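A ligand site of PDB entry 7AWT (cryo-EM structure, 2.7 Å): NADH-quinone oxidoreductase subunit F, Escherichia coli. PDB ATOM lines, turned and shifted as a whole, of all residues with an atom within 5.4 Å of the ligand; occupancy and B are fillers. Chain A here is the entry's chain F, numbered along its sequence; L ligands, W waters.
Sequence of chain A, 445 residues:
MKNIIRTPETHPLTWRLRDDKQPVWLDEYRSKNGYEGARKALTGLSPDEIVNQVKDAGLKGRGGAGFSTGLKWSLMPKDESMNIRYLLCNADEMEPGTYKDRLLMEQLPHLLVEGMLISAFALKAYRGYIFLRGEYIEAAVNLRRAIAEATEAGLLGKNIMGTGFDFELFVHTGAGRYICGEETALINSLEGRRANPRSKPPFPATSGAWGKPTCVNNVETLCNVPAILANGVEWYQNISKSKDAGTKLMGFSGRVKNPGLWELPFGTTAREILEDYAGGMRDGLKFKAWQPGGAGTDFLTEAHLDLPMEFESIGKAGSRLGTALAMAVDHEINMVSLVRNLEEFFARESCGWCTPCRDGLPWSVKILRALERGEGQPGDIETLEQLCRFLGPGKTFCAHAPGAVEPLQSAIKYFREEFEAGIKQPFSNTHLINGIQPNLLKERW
Residues that only touch the ligand: Gly 61, Arg 62, Gly 64, Ala 65, Lys 72, Glu 93, Tyr 178, Gly 181, Glu 182, Val 216, Asn 217, Ala 399 and His 400.
Hydrophobic or aromatic side chains within 4 Å of the ligand: Ala 65, Tyr 178, Ala 399 and His 400.
Of the 30 residues printed, 20 come within 4 Å of the ligand.
An oxygen (O2) of the ligand is in hydrogen-bond range of the backbone NH (N) of Met 94 (3.3 Å).
An oxygen (O9) of the ligand is in hydrogen-bond range of the side-chain hydroxyl (OG1) of Thr 221.
O7 of the ligand is in hydrogen-bond range of N of Gly 63, at 2.9 Å.
A nitrogen (N2) of the ligand lies within hydrogen-bond range of the backbone carbonyl oxygen of Asp 92 (3.2 Å).
The backbone NH of Asn 218 sits at hydrogen-bond distance from an oxygen (O9) of the ligand, at 3.1 Å.
The side-chain amide nitrogen (ND2) of Asn 90 is in hydrogen-bond range of an oxygen (O5) of the ligand, 2.8 Å away.
The backbone NH (N) of Glu 183 is in hydrogen-bond range of an oxygen (O3) of the ligand, 2.8 Å away.
The side-chain amide oxygen (OD1) of Asn 218 lies close to an oxygen (O1) of the ligand (2.6 Å).
Water W1 lies within hydrogen-bond range of O4 of the ligand and OE1 of Glu 183.
Water W2 bridges O3 of the ligand (3.0 Å) and OE1 of Glu 182 (3.4 Å).
The side-chain amide nitrogen (ND2) of Asn 218 is in hydrogen-bond range of the backbone carbonyl oxygen (O) of Arg 62, at 3.4 Å.
O of Val 216 is in hydrogen-bond range of NZ of Lys 72, at 3.4 Å.
The side-chain hydroxyl (OH) of Tyr 178 is in hydrogen-bond range of the side-chain carboxylate (OE1) of Glu 95 (3.0 Å).
N of Asn 90 is in hydrogen-bond range of O of Asn 217 (2.6 Å).
The backbone NH (N) of His 400 lies close to the side-chain sulfur (SG) of Cys 398 (3.0 Å).
The side-chain hydroxyl (OG1) of Thr 221 is in hydrogen-bond range of the backbone NH (N) of Arg 62.
The side-chain sulfur (SD) of Met 94 sits at hydrogen-bond distance from the backbone NH (N) of Tyr 178 (3.6 Å).
N of Gly 61 lies within hydrogen-bond range of O of Phe 67.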
ATOM      1  N   LYS A  60      -1.627  26.895  15.927  1.00  0.00           N
ATOM      2  CA  LYS A  60      -1.723  26.832  17.375  1.00  0.00           C
ATOM      3  C   LYS A  60      -0.359  26.899  18.030  1.00  0.00           C
ATOM      4  O   LYS A  60       0.631  26.578  17.425  1.00  0.00           O
ATOM      5  CB  LYS A  60      -2.431  25.573  17.821  1.00  0.00           C
ATOM      6  CG  LYS A  60      -3.934  25.693  17.767  1.00  0.00           C
ATOM      7  CD  LYS A  60      -4.596  24.487  18.380  1.00  0.00           C
ATOM      8  CE  LYS A  60      -5.870  24.146  17.643  1.00  0.00           C
ATOM      9  NZ  LYS A  60      -6.675  25.366  17.389  1.00  0.00           N
ATOM     10  N   GLY A  61      -0.315  27.311  19.283  1.00  0.00           N
ATOM     11  CA  GLY A  61       0.957  27.493  19.952  1.00  0.00           C
ATOM     12  C   GLY A  61       1.796  26.238  19.983  1.00  0.00           C
ATOM     13  O   GLY A  61       1.385  25.222  20.539  1.00  0.00           O
ATOM     14  N   ARG A  62       2.977  26.320  19.422  1.00  0.00           N
ATOM     15  CA  ARG A  62       3.882  25.223  19.363  1.00  0.00           C
ATOM     16  C   ARG A  62       4.823  25.136  20.515  1.00  0.00           C
ATOM     17  O   ARG A  62       5.606  24.254  20.578  1.00  0.00           O
ATOM     18  CB  ARG A  62       4.691  25.340  18.122  1.00  0.00           C
ATOM     19  CG  ARG A  62       4.286  24.367  17.060  1.00  0.00           C
ATOM     20  CD  ARG A  62       2.902  24.618  16.574  1.00  0.00           C
ATOM     21  NE  ARG A  62       2.797  24.172  15.215  1.00  0.00           N
ATOM     22  CZ  ARG A  62       1.684  23.833  14.651  1.00  0.00           C
ATOM     23  NH1 ARG A  62       0.566  23.869  15.322  1.00  0.00           N
ATOM     24  NH2 ARG A  62       1.684  23.440  13.414  1.00  0.00           N
ATOM     25  N   GLY A  63       4.769  26.065  21.437  1.00  0.00           N
ATOM     26  CA  GLY A  63       5.678  26.072  22.569  1.00  0.00           C
ATOM     27  C   GLY A  63       5.344  25.044  23.628  1.00  0.00           C
ATOM     28  O   GLY A  63       6.225  24.622  24.380  1.00  0.00           O
ATOM     29  N   GLY A  64       4.080  24.642  23.709  1.00  0.00           N
ATOM     30  CA  GLY A  64       3.673  23.670  24.711  1.00  0.00           C
ATOM     31  C   GLY A  64       2.312  23.983  25.304  1.00  0.00           C
ATOM     32  O   GLY A  64       1.619  23.089  25.795  1.00  0.00           O
ATOM     33  N   ALA A  65       1.915  25.254  25.245  1.00  0.00           N
ATOM     34  CA  ALA A  65       0.621  25.650  25.778  1.00  0.00           C
ATOM     35  C   ALA A  65      -0.505  25.166  24.868  1.00  0.00           C
ATOM     36  O   ALA A  65      -1.502  24.600  25.346  1.00  0.00           O
ATOM     37  CB  ALA A  65       0.553  27.163  25.957  1.00  0.00           C
ATOM     38  N   GLY A  66      -0.380  25.391  23.572  1.00  0.00           N
ATOM     39  CA  GLY A  66      -1.373  24.961  22.613  1.00  0.00           C
ATOM     40  C   GLY A  66      -2.438  25.987  22.275  1.00  0.00           C
ATOM     41  O   GLY A  66      -3.392  25.644  21.566  1.00  0.00           O
ATOM     42  N   PHE A  67      -2.311  27.209  22.759  1.00  0.00           N
ATOM     43  CA  PHE A  67      -3.325  28.224  22.491  1.00  0.00           C
ATOM     44  C   PHE A  67      -3.254  28.687  21.043  1.00  0.00           C
ATOM     45  O   PHE A  67      -2.212  28.597  20.387  1.00  0.00           O
ATOM     46  CB  PHE A  67      -3.141  29.423  23.428  1.00  0.00           C
ATOM     47  CG  PHE A  67      -3.296  29.075  24.870  1.00  0.00           C
ATOM     48  CD1 PHE A  67      -4.217  28.134  25.282  1.00  0.00           C
ATOM     49  CD2 PHE A  67      -2.510  29.702  25.835  1.00  0.00           C
ATOM     50  CE1 PHE A  67      -4.353  27.804  26.615  1.00  0.00           C
ATOM     51  CE2 PHE A  67      -2.643  29.382  27.169  1.00  0.00           C
ATOM     52  CZ  PHE A  67      -3.569  28.434  27.558  1.00  0.00           C
ATOM     53  N   THR A  69      -2.863  30.930  17.871  1.00  0.00           N
ATOM     54  CA  THR A  69      -2.011  32.083  17.588  1.00  0.00           C
ATOM     55  C   THR A  69      -2.821  33.252  17.045  1.00  0.00           C
ATOM     56  O   THR A  69      -2.530  34.417  17.383  1.00  0.00           O
ATOM     57  CB  THR A  69      -0.916  31.683  16.605  1.00  0.00           C
ATOM     58  OG1 THR A  69       0.055  30.873  17.274  1.00  0.00           O
ATOM     59  CG2 THR A  69      -0.222  32.888  16.025  1.00  0.00           C
ATOM     60  N   LYS A  72      -4.325  34.946  19.947  1.00  0.00           N
ATOM     61  CA  LYS A  72      -3.227  35.607  20.640  1.00  0.00           C
ATOM     62  C   LYS A  72      -2.915  36.955  20.015  1.00  0.00           C
ATOM     63  O   LYS A  72      -2.752  37.957  20.718  1.00  0.00           O
ATOM     64  CB  LYS A  72      -1.987  34.712  20.607  1.00  0.00           C
ATOM     65  CG  LYS A  72      -1.241  34.573  21.933  1.00  0.00           C
ATOM     66  CD  LYS A  72       0.068  33.825  21.726  1.00  0.00           C
ATOM     67  CE  LYS A  72       0.599  33.265  23.032  1.00  0.00           C
ATOM     68  NZ  LYS A  72       0.953  34.334  24.004  1.00  0.00           N
ATOM     69  N   ASN A  90      10.389  33.269  21.502  1.00  0.00           N
ATOM     70  CA  ASN A  90      10.822  32.521  22.674  1.00  0.00           C
ATOM     71  C   ASN A  90      11.800  31.435  22.250  1.00  0.00           C
ATOM     72  O   ASN A  90      11.503  30.244  22.259  1.00  0.00           O
ATOM     73  CB  ASN A  90       9.624  31.946  23.410  1.00  0.00           C
ATOM     74  CG  ASN A  90       9.900  31.705  24.867  1.00  0.00           C
ATOM     75  OD1 ASN A  90      11.044  31.504  25.261  1.00  0.00           O
ATOM     76  ND2 ASN A  90       8.857  31.715  25.680  1.00  0.00           N
ATOM     77  N   ASP A  92      14.435  30.779  23.894  1.00  0.00           N
ATOM     78  CA  ASP A  92      14.902  30.111  25.101  1.00  0.00           C
ATOM     79  C   ASP A  92      14.212  28.762  25.192  1.00  0.00           C
ATOM     80  O   ASP A  92      13.036  28.690  25.555  1.00  0.00           O
ATOM     81  CB  ASP A  92      14.611  30.941  26.341  1.00  0.00           C
ATOM     82  CG  ASP A  92      14.949  30.225  27.629  1.00  0.00           C
ATOM     83  OD1 ASP A  92      14.192  29.315  28.035  1.00  0.00           O
ATOM     84  OD2 ASP A  92      15.975  30.568  28.258  1.00  0.00           O
ATOM     85  N   GLU A  93      14.924  27.693  24.856  1.00  0.00           N
ATOM     86  CA  GLU A  93      14.340  26.366  24.783  1.00  0.00           C
ATOM     87  C   GLU A  93      14.979  25.502  25.866  1.00  0.00           C
ATOM     88  O   GLU A  93      15.927  24.757  25.629  1.00  0.00           O
ATOM     89  CB  GLU A  93      14.548  25.779  23.413  1.00  0.00           C
ATOM     90  CG  GLU A  93      13.936  24.431  23.214  1.00  0.00           C
ATOM     91  CD  GLU A  93      14.678  23.629  22.184  1.00  0.00           C
ATOM     92  OE1 GLU A  93      15.817  24.018  21.847  1.00  0.00           O
ATOM     93  OE2 GLU A  93      14.135  22.606  21.708  1.00  0.00           O
ATOM     94  N   MET A  94      14.425  25.605  27.062  1.00  0.00           N
ATOM     95  CA  MET A  94      14.836  24.774  28.194  1.00  0.00           C
ATOM     96  C   MET A  94      13.641  23.934  28.597  1.00  0.00           C
ATOM     97  O   MET A  94      12.617  24.469  29.036  1.00  0.00           O
ATOM     98  CB  MET A  94      15.326  25.631  29.357  1.00  0.00           C
ATOM     99  CG  MET A  94      16.589  26.388  29.071  1.00  0.00           C
ATOM    100  SD  MET A  94      17.510  26.809  30.555  1.00  0.00           S
ATOM    101  CE  MET A  94      18.819  27.779  29.834  1.00  0.00           C
ATOM    102  N   GLU A  95      13.721  22.625  28.332  1.00  0.00           N
ATOM    103  CA  GLU A  95      12.765  21.586  28.761  1.00  0.00           C
ATOM    104  C   GLU A  95      13.480  20.242  28.663  1.00  0.00           C
ATOM    105  O   GLU A  95      13.797  19.812  27.589  1.00  0.00           O
ATOM    106  CB  GLU A  95      11.516  21.573  27.913  1.00  0.00           C
ATOM    107  CG  GLU A  95      10.370  22.370  28.516  1.00  0.00           C
ATOM    108  CD  GLU A  95       9.477  21.543  29.427  1.00  0.00           C
ATOM    109  OE1 GLU A  95       9.500  21.798  30.637  1.00  0.00           O
ATOM    110  OE2 GLU A  95       8.767  20.647  28.938  1.00  0.00           O
ATOM    111  N   ASP A 101      13.921  23.535  18.572  1.00  0.00           N
ATOM    112  CA  ASP A 101      14.266  24.879  18.107  1.00  0.00           C
ATOM    113  C   ASP A 101      15.732  24.964  17.708  1.00  0.00           C
ATOM    114  O   ASP A 101      16.086  25.777  16.853  1.00  0.00           O
ATOM    115  CB  ASP A 101      13.946  25.901  19.182  1.00  0.00           C
ATOM    116  CG  ASP A 101      12.560  25.735  19.756  1.00  0.00           C
ATOM    117  OD1 ASP A 101      11.710  25.135  19.066  1.00  0.00           O
ATOM    118  OD2 ASP A 101      12.309  26.193  20.885  1.00  0.00           O
ATOM    119  N   TYR A 178      15.766  28.030  33.500  1.00  0.00           N
ATOM    120  CA  TYR A 178      14.669  27.437  32.767  1.00  0.00           C
ATOM    121  C   TYR A 178      13.385  28.236  32.910  1.00  0.00           C
ATOM    122  O   TYR A 178      12.534  28.211  32.009  1.00  0.00           O
ATOM    123  CB  TYR A 178      14.450  25.998  33.232  1.00  0.00           C
ATOM    124  CG  TYR A 178      13.052  25.469  33.084  1.00  0.00           C
ATOM    125  CD1 TYR A 178      12.547  25.143  31.842  1.00  0.00           C
ATOM    126  CD2 TYR A 178      12.243  25.263  34.185  1.00  0.00           C
ATOM    127  CE1 TYR A 178      11.270  24.655  31.695  1.00  0.00           C
ATOM    128  CE2 TYR A 178      10.971  24.773  34.051  1.00  0.00           C
ATOM    129  CZ  TYR A 178      10.486  24.473  32.806  1.00  0.00           C
ATOM    130  OH  TYR A 178       9.216  23.973  32.660  1.00  0.00           O
ATOM    131  N   ILE A 179      13.222  28.966  34.012  1.00  0.00           N
ATOM    132  CA  ILE A 179      11.985  29.692  34.244  1.00  0.00           C
ATOM    133  C   ILE A 179      11.836  30.884  33.296  1.00  0.00           C
ATOM    134  O   ILE A 179      10.718  31.367  33.098  1.00  0.00           O
ATOM    135  CB  ILE A 179      11.913  30.119  35.721  1.00  0.00           C
ATOM    136  CG1 ILE A 179      10.518  30.646  36.052  1.00  0.00           C
ATOM    137  CG2 ILE A 179      12.962  31.145  36.034  1.00  0.00           C
ATOM    138  CD1 ILE A 179       9.435  29.612  35.992  1.00  0.00           C
ATOM    139  N   GLY A 181      11.818  30.712  30.279  1.00  0.00           N
ATOM    140  CA  GLY A 181      11.023  30.272  29.146  1.00  0.00           C
ATOM    141  C   GLY A 181       9.554  30.612  29.277  1.00  0.00           C
ATOM    142  O   GLY A 181       8.864  30.671  28.265  1.00  0.00           O
ATOM    143  N   GLU A 182       9.075  30.817  30.502  1.00  0.00           N
ATOM    144  CA  GLU A 182       7.691  31.187  30.728  1.00  0.00           C
ATOM    145  C   GLU A 182       7.333  32.426  29.920  1.00  0.00           C
ATOM    146  O   GLU A 182       8.161  33.299  29.687  1.00  0.00           O
ATOM    147  CB  GLU A 182       7.459  31.446  32.209  1.00  0.00           C
ATOM    148  CG  GLU A 182       6.151  30.892  32.738  1.00  0.00           C
ATOM    149  CD  GLU A 182       5.017  31.862  32.587  1.00  0.00           C
ATOM    150  OE1 GLU A 182       3.847  31.455  32.775  1.00  0.00           O
ATOM    151  OE2 GLU A 182       5.286  33.034  32.261  1.00  0.00           O
ATOM    152  N   GLU A 183       6.077  32.485  29.474  1.00  0.00           N
ATOM    153  CA  GLU A 183       5.657  33.563  28.578  1.00  0.00           C
ATOM    154  C   GLU A 183       5.887  34.930  29.206  1.00  0.00           C
ATOM    155  O   GLU A 183       6.433  35.826  28.568  1.00  0.00           O
ATOM    156  CB  GLU A 183       4.185  33.388  28.211  1.00  0.00           C
ATOM    157  CG  GLU A 183       3.513  34.676  27.782  1.00  0.00           C
ATOM    158  CD  GLU A 183       2.143  34.468  27.185  1.00  0.00           C
ATOM    159  OE1 GLU A 183       2.048  33.854  26.101  1.00  0.00           O
ATOM    160  OE2 GLU A 183       1.150  34.903  27.802  1.00  0.00           O
ATOM    161  N   THR A 184       5.478  35.104  30.455  1.00  0.00           N
ATOM    162  CA  THR A 184       5.539  36.407  31.108  1.00  0.00           C
ATOM    163  C   THR A 184       6.700  36.532  32.086  1.00  0.00           C
ATOM    164  O   THR A 184       6.835  37.580  32.717  1.00  0.00           O
ATOM    165  CB  THR A 184       4.218  36.697  31.819  1.00  0.00           C
ATOM    166  OG1 THR A 184       3.962  35.680  32.789  1.00  0.00           O
ATOM    167  CG2 THR A 184       3.078  36.744  30.831  1.00  0.00           C
ATOM    168  N   VAL A 216       4.286  37.143  22.819  1.00  0.00           N
ATOM    169  CA  VAL A 216       5.407  36.213  22.914  1.00  0.00           C
ATOM    170  C   VAL A 216       5.051  34.944  22.160  1.00  0.00           C
ATOM    171  O   VAL A 216       4.021  34.304  22.444  1.00  0.00           O
ATOM    172  CB  VAL A 216       5.734  35.904  24.387  1.00  0.00           C
ATOM    173  CG1 VAL A 216       6.782  34.828  24.475  1.00  0.00           C
ATOM    174  CG2 VAL A 216       6.195  37.163  25.083  1.00  0.00           C
ATOM    175  N   ASN A 217       5.882  34.567  21.202  1.00  0.00           N
ATOM    176  CA  ASN A 217       5.639  33.381  20.382  1.00  0.00           C
ATOM    177  C   ASN A 217       6.886  32.512  20.384  1.00  0.00           C
ATOM    178  O   ASN A 217       8.001  32.994  20.486  1.00  0.00           O
ATOM    179  CB  ASN A 217       5.261  33.759  18.956  1.00  0.00           C
ATOM    180  CG  ASN A 217       3.804  34.126  18.817  1.00  0.00           C
ATOM    181  OD1 ASN A 217       3.464  35.166  18.266  1.00  0.00           O
ATOM    182  ND2 ASN A 217       2.929  33.275  19.332  1.00  0.00           N
ATOM    183  N   ASN A 218       6.672  31.215  20.219  1.00  0.00           N
ATOM    184  CA  ASN A 218       7.759  30.255  20.195  1.00  0.00           C
ATOM    185  C   ASN A 218       8.495  30.368  18.875  1.00  0.00           C
ATOM    186  O   ASN A 218       8.198  31.237  18.081  1.00  0.00           O
ATOM    187  CB  ASN A 218       7.197  28.859  20.319  1.00  0.00           C
ATOM    188  CG  ASN A 218       8.268  27.843  20.553  1.00  0.00           C
ATOM    189  OD1 ASN A 218       9.336  28.161  21.037  1.00  0.00           O
ATOM    190  ND2 ASN A 218       7.974  26.606  20.223  1.00  0.00           N
ATOM    191  N   VAL A 219       9.456  29.484  18.640  1.00  0.00           N
ATOM    192  CA  VAL A 219      10.204  29.525  17.386  1.00  0.00           C
ATOM    193  C   VAL A 219       9.434  28.826  16.278  1.00  0.00           C
ATOM    194  O   VAL A 219       9.361  29.322  15.151  1.00  0.00           O
ATOM    195  CB  VAL A 219      11.589  28.901  17.579  1.00  0.00           C
ATOM    196  CG1 VAL A 219      12.367  28.950  16.273  1.00  0.00           C
ATOM    197  CG2 VAL A 219      12.336  29.617  18.670  1.00  0.00           C
ATOM    198  N   THR A 221       6.218  28.248  15.984  1.00  0.00           N
ATOM    199  CA  THR A 221       5.010  28.917  15.631  1.00  0.00           C
ATOM    200  C   THR A 221       5.360  29.942  14.652  1.00  0.00           C
ATOM    201  O   THR A 221       4.805  30.031  13.624  1.00  0.00           O
ATOM    202  CB  THR A 221       4.490  29.690  16.790  1.00  0.00           C
ATOM    203  OG1 THR A 221       4.234  28.799  17.836  1.00  0.00           O
ATOM    204  CG2 THR A 221       3.258  30.313  16.438  1.00  0.00           C
ATOM    205  N   CYS A 398       2.567  30.339  38.808  1.00  0.00           N
ATOM    206  CA  CYS A 398       2.778  30.110  37.383  1.00  0.00           C
ATOM    207  C   CYS A 398       2.559  28.664  37.075  1.00  0.00           C
ATOM    208  O   CYS A 398       2.102  27.911  37.895  1.00  0.00           O
ATOM    209  CB  CYS A 398       4.163  30.542  36.942  1.00  0.00           C
ATOM    210  SG  CYS A 398       5.359  29.229  37.129  1.00  0.00           S
ATOM    211  N   ALA A 399       2.867  28.262  35.860  1.00  0.00           N
ATOM    212  CA  ALA A 399       2.639  26.901  35.455  1.00  0.00           C
ATOM    213  C   ALA A 399       3.817  25.978  35.644  1.00  0.00           C
ATOM    214  O   ALA A 399       3.798  24.885  35.148  1.00  0.00           O
ATOM    215  CB  ALA A 399       2.197  26.861  34.019  1.00  0.00           C
ATOM    216  N   HIS A 400       4.864  26.414  36.325  1.00  0.00           N
ATOM    217  CA  HIS A 400       6.047  25.585  36.485  1.00  0.00           C
ATOM    218  C   HIS A 400       5.792  24.407  37.409  1.00  0.00           C
ATOM    219  O   HIS A 400       6.198  23.277  37.113  1.00  0.00           O
ATOM    220  CB  HIS A 400       7.211  26.434  37.014  1.00  0.00           C
ATOM    221  CG  HIS A 400       8.377  25.626  37.498  1.00  0.00           C
ATOM    222  ND1 HIS A 400       9.272  25.025  36.642  1.00  0.00           N
ATOM    223  CD2 HIS A 400       8.813  25.346  38.745  1.00  0.00           C
ATOM    224  CE1 HIS A 400      10.196  24.390  37.341  1.00  0.00           C
ATOM    225  NE2 HIS A 400       9.934  24.575  38.620  1.00  0.00           N
HETATM  226  N1  LIG L   1       7.836  27.878  25.571  1.00  0.00           N
HETATM  227  C1  LIG L   1       8.916  27.746  24.737  1.00  0.00           C
HETATM  228  O1  LIG L   1       8.776  27.944  23.549  1.00  0.00           O
HETATM  229  N2  LIG L   1      10.149  27.408  25.233  1.00  0.00           N
HETATM  230  C2  LIG L   1      10.297  27.200  26.582  1.00  0.00           C
HETATM  231  O2  LIG L   1      11.372  26.894  27.056  1.00  0.00           O
HETATM  232  C3  LIG L   1       9.202  27.325  27.422  1.00  0.00           C
HETATM  233  N3  LIG L   1       9.372  27.103  28.758  1.00  0.00           N
HETATM  234  C4  LIG L   1       8.307  27.230  29.608  1.00  0.00           C
HETATM  235  C5  LIG L   1       8.541  27.002  30.944  1.00  0.00           C
HETATM  236  C6  LIG L   1       7.491  27.110  31.831  1.00  0.00           C
HETATM  237  C7  LIG L   1       7.749  26.865  33.271  1.00  0.00           C
HETATM  238  C8  LIG L   1       6.225  27.463  31.377  1.00  0.00           C
HETATM  239  C9  LIG L   1       5.079  27.578  32.326  1.00  0.00           C
HETATM  240  C10 LIG L   1       6.007  27.688  30.025  1.00  0.00           C
HETATM  241  C11 LIG L   1       7.058  27.571  29.128  1.00  0.00           C
HETATM  242  N4  LIG L   1       6.888  27.805  27.771  1.00  0.00           N
HETATM  243  C12 LIG L   1       7.959  27.666  26.923  1.00  0.00           C
HETATM  244  C13 LIG L   1       5.551  28.189  27.198  1.00  0.00           C
HETATM  245  C14 LIG L   1       5.502  29.722  27.150  1.00  0.00           C
HETATM  246  O3  LIG L   1       4.953  30.218  28.346  1.00  0.00           O
HETATM  247  C15 LIG L   1       4.700  30.305  25.983  1.00  0.00           C
HETATM  248  O4  LIG L   1       3.388  29.805  26.025  1.00  0.00           O
HETATM  249  C16 LIG L   1       5.356  29.951  24.658  1.00  0.00           C
HETATM  250  O5  LIG L   1       6.750  30.094  24.744  1.00  0.00           O
HETATM  251  C17 LIG L   1       4.863  30.835  23.521  1.00  0.00           C
HETATM  252  O6  LIG L   1       3.492  30.593  23.346  1.00  0.00           O
HETATM  253  P1  LIG L   1       2.995  29.760  22.064  1.00  0.00           P
HETATM  254  O7  LIG L   1       3.159  28.302  22.387  1.00  0.00           O
HETATM  255  O8  LIG L   1       1.554  30.078  21.771  1.00  0.00           O
HETATM  256  O9  LIG L   1       3.847  30.098  20.885  1.00  0.00           O
HETATM  257  O   HOH W   1       0.704  30.835  26.289  1.00  0.00           O
HETATM  258  O   HOH W   2       2.662  29.477  30.213  1.00  0.00           O
